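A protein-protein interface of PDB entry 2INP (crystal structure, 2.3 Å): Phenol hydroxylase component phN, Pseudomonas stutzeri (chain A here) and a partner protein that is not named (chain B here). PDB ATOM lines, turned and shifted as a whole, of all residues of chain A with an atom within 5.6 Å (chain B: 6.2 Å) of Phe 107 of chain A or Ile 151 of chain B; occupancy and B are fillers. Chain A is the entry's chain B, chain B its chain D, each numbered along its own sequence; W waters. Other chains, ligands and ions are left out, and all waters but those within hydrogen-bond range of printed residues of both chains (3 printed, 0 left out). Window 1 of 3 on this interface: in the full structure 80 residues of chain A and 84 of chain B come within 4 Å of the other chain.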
ATOM      1  N   LEU A 102      35.421   7.474  -2.954  1.00  0.00           N
ATOM      2  CA  LEU A 102      34.436   8.082  -1.990  1.00  0.00           C
ATOM      3  C   LEU A 102      33.888   9.435  -2.445  1.00  0.00           C
ATOM      4  O   LEU A 102      32.777   9.860  -2.054  1.00  0.00           O
ATOM      5  CB  LEU A 102      35.131   8.207  -0.626  1.00  0.00           C
ATOM      6  CG  LEU A 102      35.169   7.044   0.373  1.00  0.00           C
ATOM      7  CD1 LEU A 102      35.001   5.652  -0.273  1.00  0.00           C
ATOM      8  CD2 LEU A 102      36.322   7.131   1.338  1.00  0.00           C
ATOM      9  N   GLU A 103      34.704  10.151  -3.227  1.00  0.00           N
ATOM     10  CA  GLU A 103      34.300  11.418  -3.868  1.00  0.00           C
ATOM     11  C   GLU A 103      33.175  11.110  -4.798  1.00  0.00           C
ATOM     12  O   GLU A 103      32.174  11.804  -4.811  1.00  0.00           O
ATOM     13  CB  GLU A 103      35.482  12.023  -4.671  1.00  0.00           C
ATOM     14  CG  GLU A 103      36.772  12.110  -3.896  1.00  0.00           C
ATOM     15  CD  GLU A 103      36.796  13.365  -3.043  1.00  0.00           C
ATOM     16  OE1 GLU A 103      35.734  14.077  -3.026  1.00  0.00           O
ATOM     17  OE2 GLU A 103      37.867  13.669  -2.450  1.00  0.00           O
ATOM     18  N   HIS A 104      33.335  10.030  -5.567  1.00  0.00           N
ATOM     19  CA  HIS A 104      32.277   9.621  -6.480  1.00  0.00           C
ATOM     20  C   HIS A 104      31.001   9.180  -5.780  1.00  0.00           C
ATOM     21  O   HIS A 104      29.869   9.594  -6.153  1.00  0.00           O
ATOM     22  CB  HIS A 104      32.760   8.537  -7.472  1.00  0.00           C
ATOM     23  CG  HIS A 104      32.118   8.674  -8.798  1.00  0.00           C
ATOM     24  ND1 HIS A 104      32.573   9.584  -9.730  1.00  0.00           N
ATOM     25  CD2 HIS A 104      30.986   8.133  -9.302  1.00  0.00           C
ATOM     26  CE1 HIS A 104      31.770   9.541 -10.791  1.00  0.00           C
ATOM     27  NE2 HIS A 104      30.823   8.643 -10.571  1.00  0.00           N
ATOM     28  N   ALA A 105      31.158   8.348  -4.749  1.00  0.00           N
ATOM     29  CA  ALA A 105      30.003   7.945  -3.900  1.00  0.00           C
ATOM     30  C   ALA A 105      29.326   9.121  -3.260  1.00  0.00           C
ATOM     31  O   ALA A 105      28.112   9.129  -3.077  1.00  0.00           O
ATOM     32  CB  ALA A 105      30.415   6.886  -2.845  1.00  0.00           C
ATOM     33  N   ALA A 106      30.097  10.120  -2.867  1.00  0.00           N
ATOM     34  CA  ALA A 106      29.493  11.348  -2.307  1.00  0.00           C
ATOM     35  C   ALA A 106      28.648  12.165  -3.361  1.00  0.00           C
ATOM     36  O   ALA A 106      27.552  12.729  -3.076  1.00  0.00           O
ATOM     37  CB  ALA A 106      30.588  12.198  -1.706  1.00  0.00           C
ATOM     38  N   PHE A 107      29.183  12.258  -4.570  1.00  0.00           N
ATOM     39  CA  PHE A 107      28.430  12.789  -5.710  1.00  0.00           C
ATOM     40  C   PHE A 107      27.044  12.104  -5.755  1.00  0.00           C
ATOM     41  O   PHE A 107      26.001  12.770  -5.711  1.00  0.00           O
ATOM     42  CB  PHE A 107      29.251  12.589  -7.036  1.00  0.00           C
ATOM     43  CG  PHE A 107      28.394  12.536  -8.285  1.00  0.00           C
ATOM     44  CD1 PHE A 107      27.594  13.650  -8.665  1.00  0.00           C
ATOM     45  CD2 PHE A 107      28.408  11.400  -9.121  1.00  0.00           C
ATOM     46  CE1 PHE A 107      26.799  13.621  -9.798  1.00  0.00           C
ATOM     47  CE2 PHE A 107      27.590  11.355 -10.273  1.00  0.00           C
ATOM     48  CZ  PHE A 107      26.794  12.491 -10.636  1.00  0.00           C
ATOM     49  N   GLN A 108      27.040  10.778  -5.817  1.00  0.00           N
ATOM     50  CA  GLN A 108      25.811  10.010  -5.829  1.00  0.00           C
ATOM     51  C   GLN A 108      24.926  10.251  -4.578  1.00  0.00           C
ATOM     52  O   GLN A 108      23.723  10.446  -4.719  1.00  0.00           O
ATOM     53  CB  GLN A 108      26.157   8.510  -5.913  1.00  0.00           C
ATOM     54  CG  GLN A 108      27.029   8.176  -7.137  1.00  0.00           C
ATOM     55  CD  GLN A 108      27.140   6.679  -7.410  1.00  0.00           C
ATOM     56  OE1 GLN A 108      27.812   5.898  -6.673  1.00  0.00           O
ATOM     57  NE2 GLN A 108      26.530   6.283  -8.505  1.00  0.00           N
ATOM     58  N   GLY A 109      25.503  10.193  -3.382  1.00  0.00           N
ATOM     59  CA  GLY A 109      24.774  10.433  -2.166  1.00  0.00           C
ATOM     60  C   GLY A 109      24.145  11.815  -2.126  1.00  0.00           C
ATOM     61  O   GLY A 109      22.957  11.925  -1.871  1.00  0.00           O
ATOM     62  N   TYR A 110      24.937  12.853  -2.394  1.00  0.00           N
ATOM     63  CA  TYR A 110      24.447  14.207  -2.387  1.00  0.00           C
ATOM     64  C   TYR A 110      23.411  14.569  -3.474  1.00  0.00           C
ATOM     65  O   TYR A 110      22.518  15.387  -3.239  1.00  0.00           O
ATOM     66  CB  TYR A 110      25.620  15.193  -2.386  1.00  0.00           C
ATOM     67  CG  TYR A 110      26.189  15.405  -0.986  1.00  0.00           C
ATOM     68  CD1 TYR A 110      27.412  14.871  -0.641  1.00  0.00           C
ATOM     69  CD2 TYR A 110      25.512  16.155  -0.032  1.00  0.00           C
ATOM     70  CE1 TYR A 110      27.957  15.016   0.624  1.00  0.00           C
ATOM     71  CE2 TYR A 110      26.085  16.398   1.281  1.00  0.00           C
ATOM     72  CZ  TYR A 110      27.286  15.776   1.596  1.00  0.00           C
ATOM     73  OH  TYR A 110      27.900  15.932   2.827  1.00  0.00           O
ATOM     74  N   SER A 111      23.579  14.000  -4.669  1.00  0.00           N
ATOM     75  CA  SER A 111      22.574  14.057  -5.737  1.00  0.00           C
ATOM     76  C   SER A 111      21.206  13.592  -5.199  1.00  0.00           C
ATOM     77  O   SER A 111      20.200  14.295  -5.349  1.00  0.00           O
ATOM     78  CB  SER A 111      22.993  13.106  -6.906  1.00  0.00           C
ATOM     79  OG  SER A 111      24.057  13.673  -7.674  1.00  0.00           O
ATOM     80  N   LYS A 112      21.174  12.390  -4.624  1.00  0.00           N
ATOM     81  CA  LYS A 112      19.953  11.852  -4.044  1.00  0.00           C
ATOM     82  C   LYS A 112      19.383  12.798  -2.951  1.00  0.00           C
ATOM     83  O   LYS A 112      18.275  13.291  -3.027  1.00  0.00           O
ATOM     84  CB  LYS A 112      20.178  10.472  -3.445  1.00  0.00           C
ATOM     85  CG  LYS A 112      18.803   9.749  -3.306  1.00  0.00           C
ATOM     86  CD  LYS A 112      18.913   8.258  -2.906  1.00  0.00           C
ATOM     87  CE  LYS A 112      17.626   7.900  -2.205  1.00  0.00           C
ATOM     88  NZ  LYS A 112      16.525   8.318  -3.110  1.00  0.00           N
ATOM     89  N   GLN A 127      22.898  19.947  -3.785  1.00  0.00           N
ATOM     90  CA  GLN A 127      23.092  19.758  -5.178  1.00  0.00           C
ATOM     91  C   GLN A 127      24.444  20.349  -5.579  1.00  0.00           C
ATOM     92  O   GLN A 127      25.125  19.774  -6.432  1.00  0.00           O
ATOM     93  CB  GLN A 127      21.990  20.409  -5.946  1.00  0.00           C
ATOM     94  CG  GLN A 127      20.747  19.584  -6.108  1.00  0.00           C
ATOM     95  CD  GLN A 127      19.596  20.409  -6.692  1.00  0.00           C
ATOM     96  OE1 GLN A 127      19.827  21.413  -7.359  1.00  0.00           O
ATOM     97  NE2 GLN A 127      18.360  19.990  -6.441  1.00  0.00           N
ATOM     98  N   ALA A 130      26.995  18.050  -4.414  1.00  0.00           N
ATOM     99  CA  ALA A 130      27.063  16.868  -5.271  1.00  0.00           C
ATOM    100  C   ALA A 130      27.992  17.132  -6.463  1.00  0.00           C
ATOM    101  O   ALA A 130      28.830  16.260  -6.855  1.00  0.00           O
ATOM    102  CB  ALA A 130      25.697  16.493  -5.763  1.00  0.00           C
ATOM    103  N   ILE A 131      27.836  18.323  -7.047  1.00  0.00           N
ATOM    104  CA  ILE A 131      28.583  18.619  -8.235  1.00  0.00           C
ATOM    105  C   ILE A 131      30.047  18.947  -7.895  1.00  0.00           C
ATOM    106  O   ILE A 131      30.937  18.608  -8.663  1.00  0.00           O
ATOM    107  CB  ILE A 131      27.850  19.689  -9.128  1.00  0.00           C
ATOM    108  CG1 ILE A 131      28.271  19.504 -10.587  1.00  0.00           C
ATOM    109  CG2 ILE A 131      27.995  21.115  -8.570  1.00  0.00           C
ATOM    110  CD1 ILE A 131      27.957  20.698 -11.515  1.00  0.00           C
ATOM    111  N   GLU A 133      31.660  17.208  -5.674  1.00  0.00           N
ATOM    112  CA  GLU A 133      32.267  15.867  -5.438  1.00  0.00           C
ATOM    113  C   GLU A 133      32.522  15.182  -6.792  1.00  0.00           C
ATOM    114  O   GLU A 133      33.475  14.431  -6.966  1.00  0.00           O
ATOM    115  CB  GLU A 133      31.362  15.064  -4.465  1.00  0.00           C
ATOM    116  CG  GLU A 133      31.074  15.759  -3.070  1.00  0.00           C
ATOM    117  CD  GLU A 133      32.266  15.823  -2.174  1.00  0.00           C
ATOM    118  OE1 GLU A 133      32.227  16.477  -1.028  1.00  0.00           O
ATOM    119  OE2 GLU A 133      33.332  15.313  -2.642  1.00  0.00           O
ATOM    120  N   LEU A 134      31.677  15.453  -7.788  1.00  0.00           N
ATOM    121  CA  LEU A 134      31.940  14.982  -9.138  1.00  0.00           C
ATOM    122  C   LEU A 134      33.238  15.627  -9.606  1.00  0.00           C
ATOM    123  O   LEU A 134      34.061  14.959 -10.213  1.00  0.00           O
ATOM    124  CB  LEU A 134      30.792  15.363 -10.098  1.00  0.00           C
ATOM    125  CG  LEU A 134      30.928  14.861 -11.521  1.00  0.00           C
ATOM    126  CD1 LEU A 134      31.246  13.368 -11.496  1.00  0.00           C
ATOM    127  CD2 LEU A 134      29.722  15.211 -12.360  1.00  0.00           C
ATOM    128  N   TYR B  81      32.464  21.500 -18.640  1.00  0.00           N
ATOM    129  CA  TYR B  81      31.128  22.004 -18.375  1.00  0.00           C
ATOM    130  C   TYR B  81      31.142  23.413 -17.759  1.00  0.00           C
ATOM    131  O   TYR B  81      30.445  24.338 -18.235  1.00  0.00           O
ATOM    132  CB  TYR B  81      30.382  21.042 -17.441  1.00  0.00           C
ATOM    133  CG  TYR B  81      29.162  21.651 -16.828  1.00  0.00           C
ATOM    134  CD1 TYR B  81      28.021  21.883 -17.595  1.00  0.00           C
ATOM    135  CD2 TYR B  81      29.130  21.989 -15.483  1.00  0.00           C
ATOM    136  CE1 TYR B  81      26.858  22.449 -16.987  1.00  0.00           C
ATOM    137  CE2 TYR B  81      27.935  22.569 -14.881  1.00  0.00           C
ATOM    138  CZ  TYR B  81      26.848  22.794 -15.638  1.00  0.00           C
ATOM    139  OH  TYR B  81      25.720  23.358 -15.074  1.00  0.00           O
ATOM    140  N   ASN B 134      15.973  16.269 -12.372  1.00  0.00           N
ATOM    141  CA  ASN B 134      17.308  15.882 -12.832  1.00  0.00           C
ATOM    142  C   ASN B 134      18.302  15.462 -11.736  1.00  0.00           C
ATOM    143  O   ASN B 134      19.180  14.608 -11.965  1.00  0.00           O
ATOM    144  CB  ASN B 134      17.854  16.990 -13.735  1.00  0.00           C
ATOM    145  CG  ASN B 134      17.206  16.963 -15.125  1.00  0.00           C
ATOM    146  OD1 ASN B 134      16.480  17.905 -15.543  1.00  0.00           O
ATOM    147  ND2 ASN B 134      17.445  15.905 -15.830  1.00  0.00           N
ATOM    148  N   ALA B 135      18.220  16.114 -10.583  1.00  0.00           N
ATOM    149  CA  ALA B 135      18.837  15.656  -9.357  1.00  0.00           C
ATOM    150  C   ALA B 135      18.470  14.207  -9.021  1.00  0.00           C
ATOM    151  O   ALA B 135      19.309  13.412  -8.696  1.00  0.00           O
ATOM    152  CB  ALA B 135      18.432  16.599  -8.170  1.00  0.00           C
ATOM    153  N   ALA B 138      20.088  12.042 -11.495  1.00  0.00           N
ATOM    154  CA  ALA B 138      21.534  11.888 -11.215  1.00  0.00           C
ATOM    155  C   ALA B 138      21.805  10.938 -10.123  1.00  0.00           C
ATOM    156  O   ALA B 138      22.927  10.430 -10.066  1.00  0.00           O
ATOM    157  CB  ALA B 138      22.244  13.184 -10.944  1.00  0.00           C
ATOM    158  N   GLY B 139      20.865  10.751  -9.185  1.00  0.00           N
ATOM    159  CA  GLY B 139      21.200   9.944  -8.038  1.00  0.00           C
ATOM    160  C   GLY B 139      20.764   8.490  -8.249  1.00  0.00           C
ATOM    161  O   GLY B 139      21.135   7.622  -7.482  1.00  0.00           O
ATOM    162  N   THR B 144      28.339   6.846 -14.888  1.00  0.00           N
ATOM    163  CA  THR B 144      28.741   8.249 -14.766  1.00  0.00           C
ATOM    164  C   THR B 144      28.400   9.047 -16.080  1.00  0.00           C
ATOM    165  O   THR B 144      28.072  10.248 -16.013  1.00  0.00           O
ATOM    166  CB  THR B 144      30.235   8.246 -14.456  1.00  0.00           C
ATOM    167  OG1 THR B 144      30.400   7.509 -13.260  1.00  0.00           O
ATOM    168  CG2 THR B 144      30.823   9.585 -14.352  1.00  0.00           C
ATOM    169  N   VAL B 146      25.892   8.968 -17.888  1.00  0.00           N
ATOM    170  CA  VAL B 146      24.479   9.319 -17.823  1.00  0.00           C
ATOM    171  C   VAL B 146      24.180  10.230 -16.596  1.00  0.00           C
ATOM    172  O   VAL B 146      23.485  11.252 -16.702  1.00  0.00           O
ATOM    173  CB  VAL B 146      23.591   8.030 -17.688  1.00  0.00           C
ATOM    174  CG1 VAL B 146      22.152   8.409 -17.591  1.00  0.00           C
ATOM    175  CG2 VAL B 146      23.841   7.038 -18.895  1.00  0.00           C
ATOM    176  N   SER B 147      24.655   9.818 -15.424  1.00  0.00           N
ATOM    177  CA  SER B 147      24.327  10.587 -14.220  1.00  0.00           C
ATOM    178  C   SER B 147      24.989  11.981 -14.283  1.00  0.00           C
ATOM    179  O   SER B 147      24.388  12.940 -13.878  1.00  0.00           O
ATOM    180  CB  SER B 147      24.754   9.817 -12.976  1.00  0.00           C
ATOM    181  OG  SER B 147      26.161   9.726 -13.046  1.00  0.00           O
ATOM    182  N   GLN B 148      26.230  12.090 -14.788  1.00  0.00           N
ATOM    183  CA  GLN B 148      26.861  13.400 -14.875  1.00  0.00           C
ATOM    184  C   GLN B 148      26.091  14.373 -15.809  1.00  0.00           C
ATOM    185  O   GLN B 148      25.939  15.508 -15.497  1.00  0.00           O
ATOM    186  CB  GLN B 148      28.316  13.261 -15.205  1.00  0.00           C
ATOM    187  CG  GLN B 148      28.729  13.758 -16.533  1.00  0.00           C
ATOM    188  CD  GLN B 148      30.199  13.582 -16.756  1.00  0.00           C
ATOM    189  OE1 GLN B 148      30.618  12.698 -17.515  1.00  0.00           O
ATOM    190  NE2 GLN B 148      31.013  14.432 -16.113  1.00  0.00           N
ATOM    191  N   MET B 149      25.466  13.899 -16.869  1.00  0.00           N
ATOM    192  CA  MET B 149      24.742  14.812 -17.764  1.00  0.00           C
ATOM    193  C   MET B 149      23.492  15.392 -17.108  1.00  0.00           C
ATOM    194  O   MET B 149      23.022  16.497 -17.446  1.00  0.00           O
ATOM    195  CB  MET B 149      24.330  14.099 -19.067  1.00  0.00           C
ATOM    196  CG  MET B 149      25.436  13.972 -20.143  1.00  0.00           C
ATOM    197  SD  MET B 149      24.905  12.886 -21.487  1.00  0.00           S
ATOM    198  CE  MET B 149      25.746  13.714 -22.708  1.00  0.00           C
ATOM    199  N   HIS B 150      22.904  14.595 -16.238  1.00  0.00           N
ATOM    200  CA  HIS B 150      21.699  14.977 -15.496  1.00  0.00           C
ATOM    201  C   HIS B 150      21.970  15.895 -14.311  1.00  0.00           C
ATOM    202  O   HIS B 150      21.170  16.779 -14.012  1.00  0.00           O
ATOM    203  CB  HIS B 150      20.929  13.696 -15.092  1.00  0.00           C
ATOM    204  CG  HIS B 150      20.247  13.021 -16.256  1.00  0.00           C
ATOM    205  ND1 HIS B 150      20.862  12.045 -17.009  1.00  0.00           N
ATOM    206  CD2 HIS B 150      19.006  13.180 -16.787  1.00  0.00           C
ATOM    207  CE1 HIS B 150      20.029  11.632 -17.957  1.00  0.00           C
ATOM    208  NE2 HIS B 150      18.894  12.299 -17.846  1.00  0.00           N
ATOM    209  N   ILE B 151      23.114  15.745 -13.665  1.00  0.00           N
ATOM    210  CA  ILE B 151      23.522  16.756 -12.702  1.00  0.00           C
ATOM    211  C   ILE B 151      23.839  18.143 -13.373  1.00  0.00           C
ATOM    212  O   ILE B 151      23.423  19.215 -12.854  1.00  0.00           O
ATOM    213  CB  ILE B 151      24.641  16.271 -11.739  1.00  0.00           C
ATOM    214  CG1 ILE B 151      24.719  17.137 -10.428  1.00  0.00           C
ATOM    215  CG2 ILE B 151      25.997  16.216 -12.425  1.00  0.00           C
ATOM    216  CD1 ILE B 151      23.400  17.154  -9.559  1.00  0.00           C
ATOM    217  N   TYR B 152      24.570  18.133 -14.493  1.00  0.00           N
ATOM    218  CA  TYR B 152      24.838  19.360 -15.220  1.00  0.00           C
ATOM    219  C   TYR B 152      23.555  19.990 -15.643  1.00  0.00           C
ATOM    220  O   TYR B 152      23.313  21.150 -15.354  1.00  0.00           O
ATOM    221  CB  TYR B 152      25.720  19.141 -16.428  1.00  0.00           C
ATOM    222  CG  TYR B 152      27.092  18.562 -16.091  1.00  0.00           C
ATOM    223  CD1 TYR B 152      27.781  17.801 -17.019  1.00  0.00           C
ATOM    224  CD2 TYR B 152      27.661  18.746 -14.829  1.00  0.00           C
ATOM    225  CE1 TYR B 152      29.026  17.255 -16.710  1.00  0.00           C
ATOM    226  CE2 TYR B 152      28.916  18.223 -14.497  1.00  0.00           C
ATOM    227  CZ  TYR B 152      29.585  17.471 -15.466  1.00  0.00           C
ATOM    228  OH  TYR B 152      30.775  16.914 -15.174  1.00  0.00           O
ATOM    229  N   THR B 153      22.678  19.254 -16.281  1.00  0.00           N
ATOM    230  CA  THR B 153      21.428  19.868 -16.733  1.00  0.00           C
ATOM    231  C   THR B 153      20.523  20.353 -15.574  1.00  0.00           C
ATOM    232  O   THR B 153      19.853  21.349 -15.758  1.00  0.00           O
ATOM    233  CB  THR B 153      20.706  19.007 -17.832  1.00  0.00           C
ATOM    234  OG1 THR B 153      19.803  19.837 -18.611  1.00  0.00           O
ATOM    235  CG2 THR B 153      19.944  17.814 -17.228  1.00  0.00           C
ATOM    236  N   GLY B 154      20.519  19.696 -14.405  1.00  0.00           N
ATOM    237  CA  GLY B 154      19.748  20.123 -13.247  1.00  0.00           C
ATOM    238  C   GLY B 154      20.213  21.452 -12.702  1.00  0.00           C
ATOM    239  O   GLY B 154      19.390  22.374 -12.461  1.00  0.00           O
ATOM    240  N   MET B 155      21.524  21.621 -12.636  1.00  0.00           N
ATOM    241  CA  MET B 155      22.097  22.904 -12.249  1.00  0.00           C
ATOM    242  C   MET B 155      21.799  23.979 -13.211  1.00  0.00           C
ATOM    243  O   MET B 155      21.540  25.104 -12.809  1.00  0.00           O
ATOM    244  CB  MET B 155      23.602  22.798 -11.985  1.00  0.00           C
ATOM    245  CG  MET B 155      23.982  21.750 -10.867  1.00  0.00           C
ATOM    246  SD  MET B 155      23.203  22.104  -9.269  1.00  0.00           S
ATOM    247  CE  MET B 155      21.810  21.060  -9.339  1.00  0.00           C
ATOM    248  N   ASP B 156      21.808  23.640 -14.516  1.00  0.00           N
ATOM    249  CA  ASP B 156      21.423  24.559 -15.580  1.00  0.00           C
ATOM    250  C   ASP B 156      19.953  25.019 -15.358  1.00  0.00           C
ATOM    251  O   ASP B 156      19.658  26.210 -15.505  1.00  0.00           O
ATOM    252  CB  ASP B 156      21.546  23.861 -16.925  1.00  0.00           C
ATOM    253  CG  ASP B 156      22.987  23.668 -17.381  1.00  0.00           C
ATOM    254  OD1 ASP B 156      23.946  24.179 -16.775  1.00  0.00           O
ATOM    255  OD2 ASP B 156      23.178  22.986 -18.419  1.00  0.00           O
HETATM  256  O   HOH W   1      24.517   7.802  -9.792  1.00  0.00           O
HETATM  257  O   HOH W   2      27.384   7.728 -11.556  1.00  0.00           O
HETATM  258  O   HOH W   3      22.447   7.937  -5.247  1.00  0.00           O
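NE2 of His 104 of chain A lies within hydrogen-bond range of OG1 of Thr 144 of chain B (2.9 Å).
The side-chain carboxylate (OD1) of Asp 156 of chain B lies within hydrogen-bond range of the side-chain hydroxyl (OH) of Tyr 81 of chain B (2.6 Å).
The backbone carbonyl oxygen (O) of Phe 107 of chain A lies within hydrogen-bond range of the side-chain hydroxyl (OG) of Ser 111 of chain A, at 2.9 Å.
OH of Tyr 152 of chain B sits at hydrogen-bond distance from NE2 of Gln 148 of chain B, 2.7 Å away.
O of Tyr 152 of chain B is in hydrogen-bond range of OH of Tyr 81 of chain B.
Among the printed residues, pairs that only touch across the chains: Gln 127 of chain A with Met 155 of chain B, Leu 134 of chain A with Tyr 152 of chain B, Phe 107 of chain A with Ser 147 of chain B, Ser 111 of chain A with Ala 135 of chain B, Leu 134 of chain A with Gln 148 of chain B, Ser 111 of chain A with Ala 138 of chain B, Phe 107 of chain A with Ile 151 of chain B, Gln 127 of chain A with Ala 135 of chain B, Ser 111 of chain A with Gly 139 of chain B, Ile 131 of chain A with Tyr 81 of chain B, Ile 131 of chain A with Tyr 152 of chain B and Leu 134 of chain A with Ile 151 of chain B.
Phe 107 of chain A touches just these residues of chain B: Ser 147 (3.5 Å) and Ile 151 (3.8 Å).
Of the printed residues of chain A, Ile 151 of chain B touches Phe 107 and Leu 134.
Printed residues of chain B within 4 Å of Gln 127 of chain A: Ala 135 (3.8 Å) and Met 155 (2.8 Å).
Of the printed residues of chain A, Tyr 81 of chain B touches Ile 131 (3.9 Å).
Glu 133 of chain A touches none of the printed residues of chain B.
Tyr 110 of chain A touches none of the printed residues of chain B.
The nearest printed residue of chain A that does not touch Ile 151 of chain B is Ser 111 of chain A (4.01 Å).
The nearest printed residue of chain A that does not touch Thr 144 of chain B is Leu 134 of chain A (4.8 Å).
Printed residues of chain B that touch a printed residue of chain A: Tyr 81, Ala 135, Ala 138, Gly 139, Thr 144, Ser 147, Gln 148, Ile 151, Tyr 152 and Met 155.
Hydrophobic or aromatic side chains of chain B that line the printed part of chain A: Tyr 81, Ala 135, Ala 138, Ile 151, Tyr 152 and Met 155.
Hydrophobic or aromatic side chains of chain A that line the printed part of chain B: His 104, Phe 107, Ile 131 and Leu 134.
Among the printed residues, 13 pairs touch across the chains.
Water W3 lies within hydrogen-bond range of the backbone carbonyl oxygen of Gly 139 of chain B and the backbone carbonyl oxygen of Gln 108 of chain A.
Water W2 lies within hydrogen-bond range of OG of Ser 147 of chain B (2.8 Å), OG1 of Thr 144 of chain B (3.5 Å) and NE2 of Gln 108 of chain A (3.5 Å).
Water W1 bridges the side-chain amide nitrogen (NE2) of Gln 108 of chain A and the backbone carbonyl oxygen (O) of Ala 138 of chain B.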
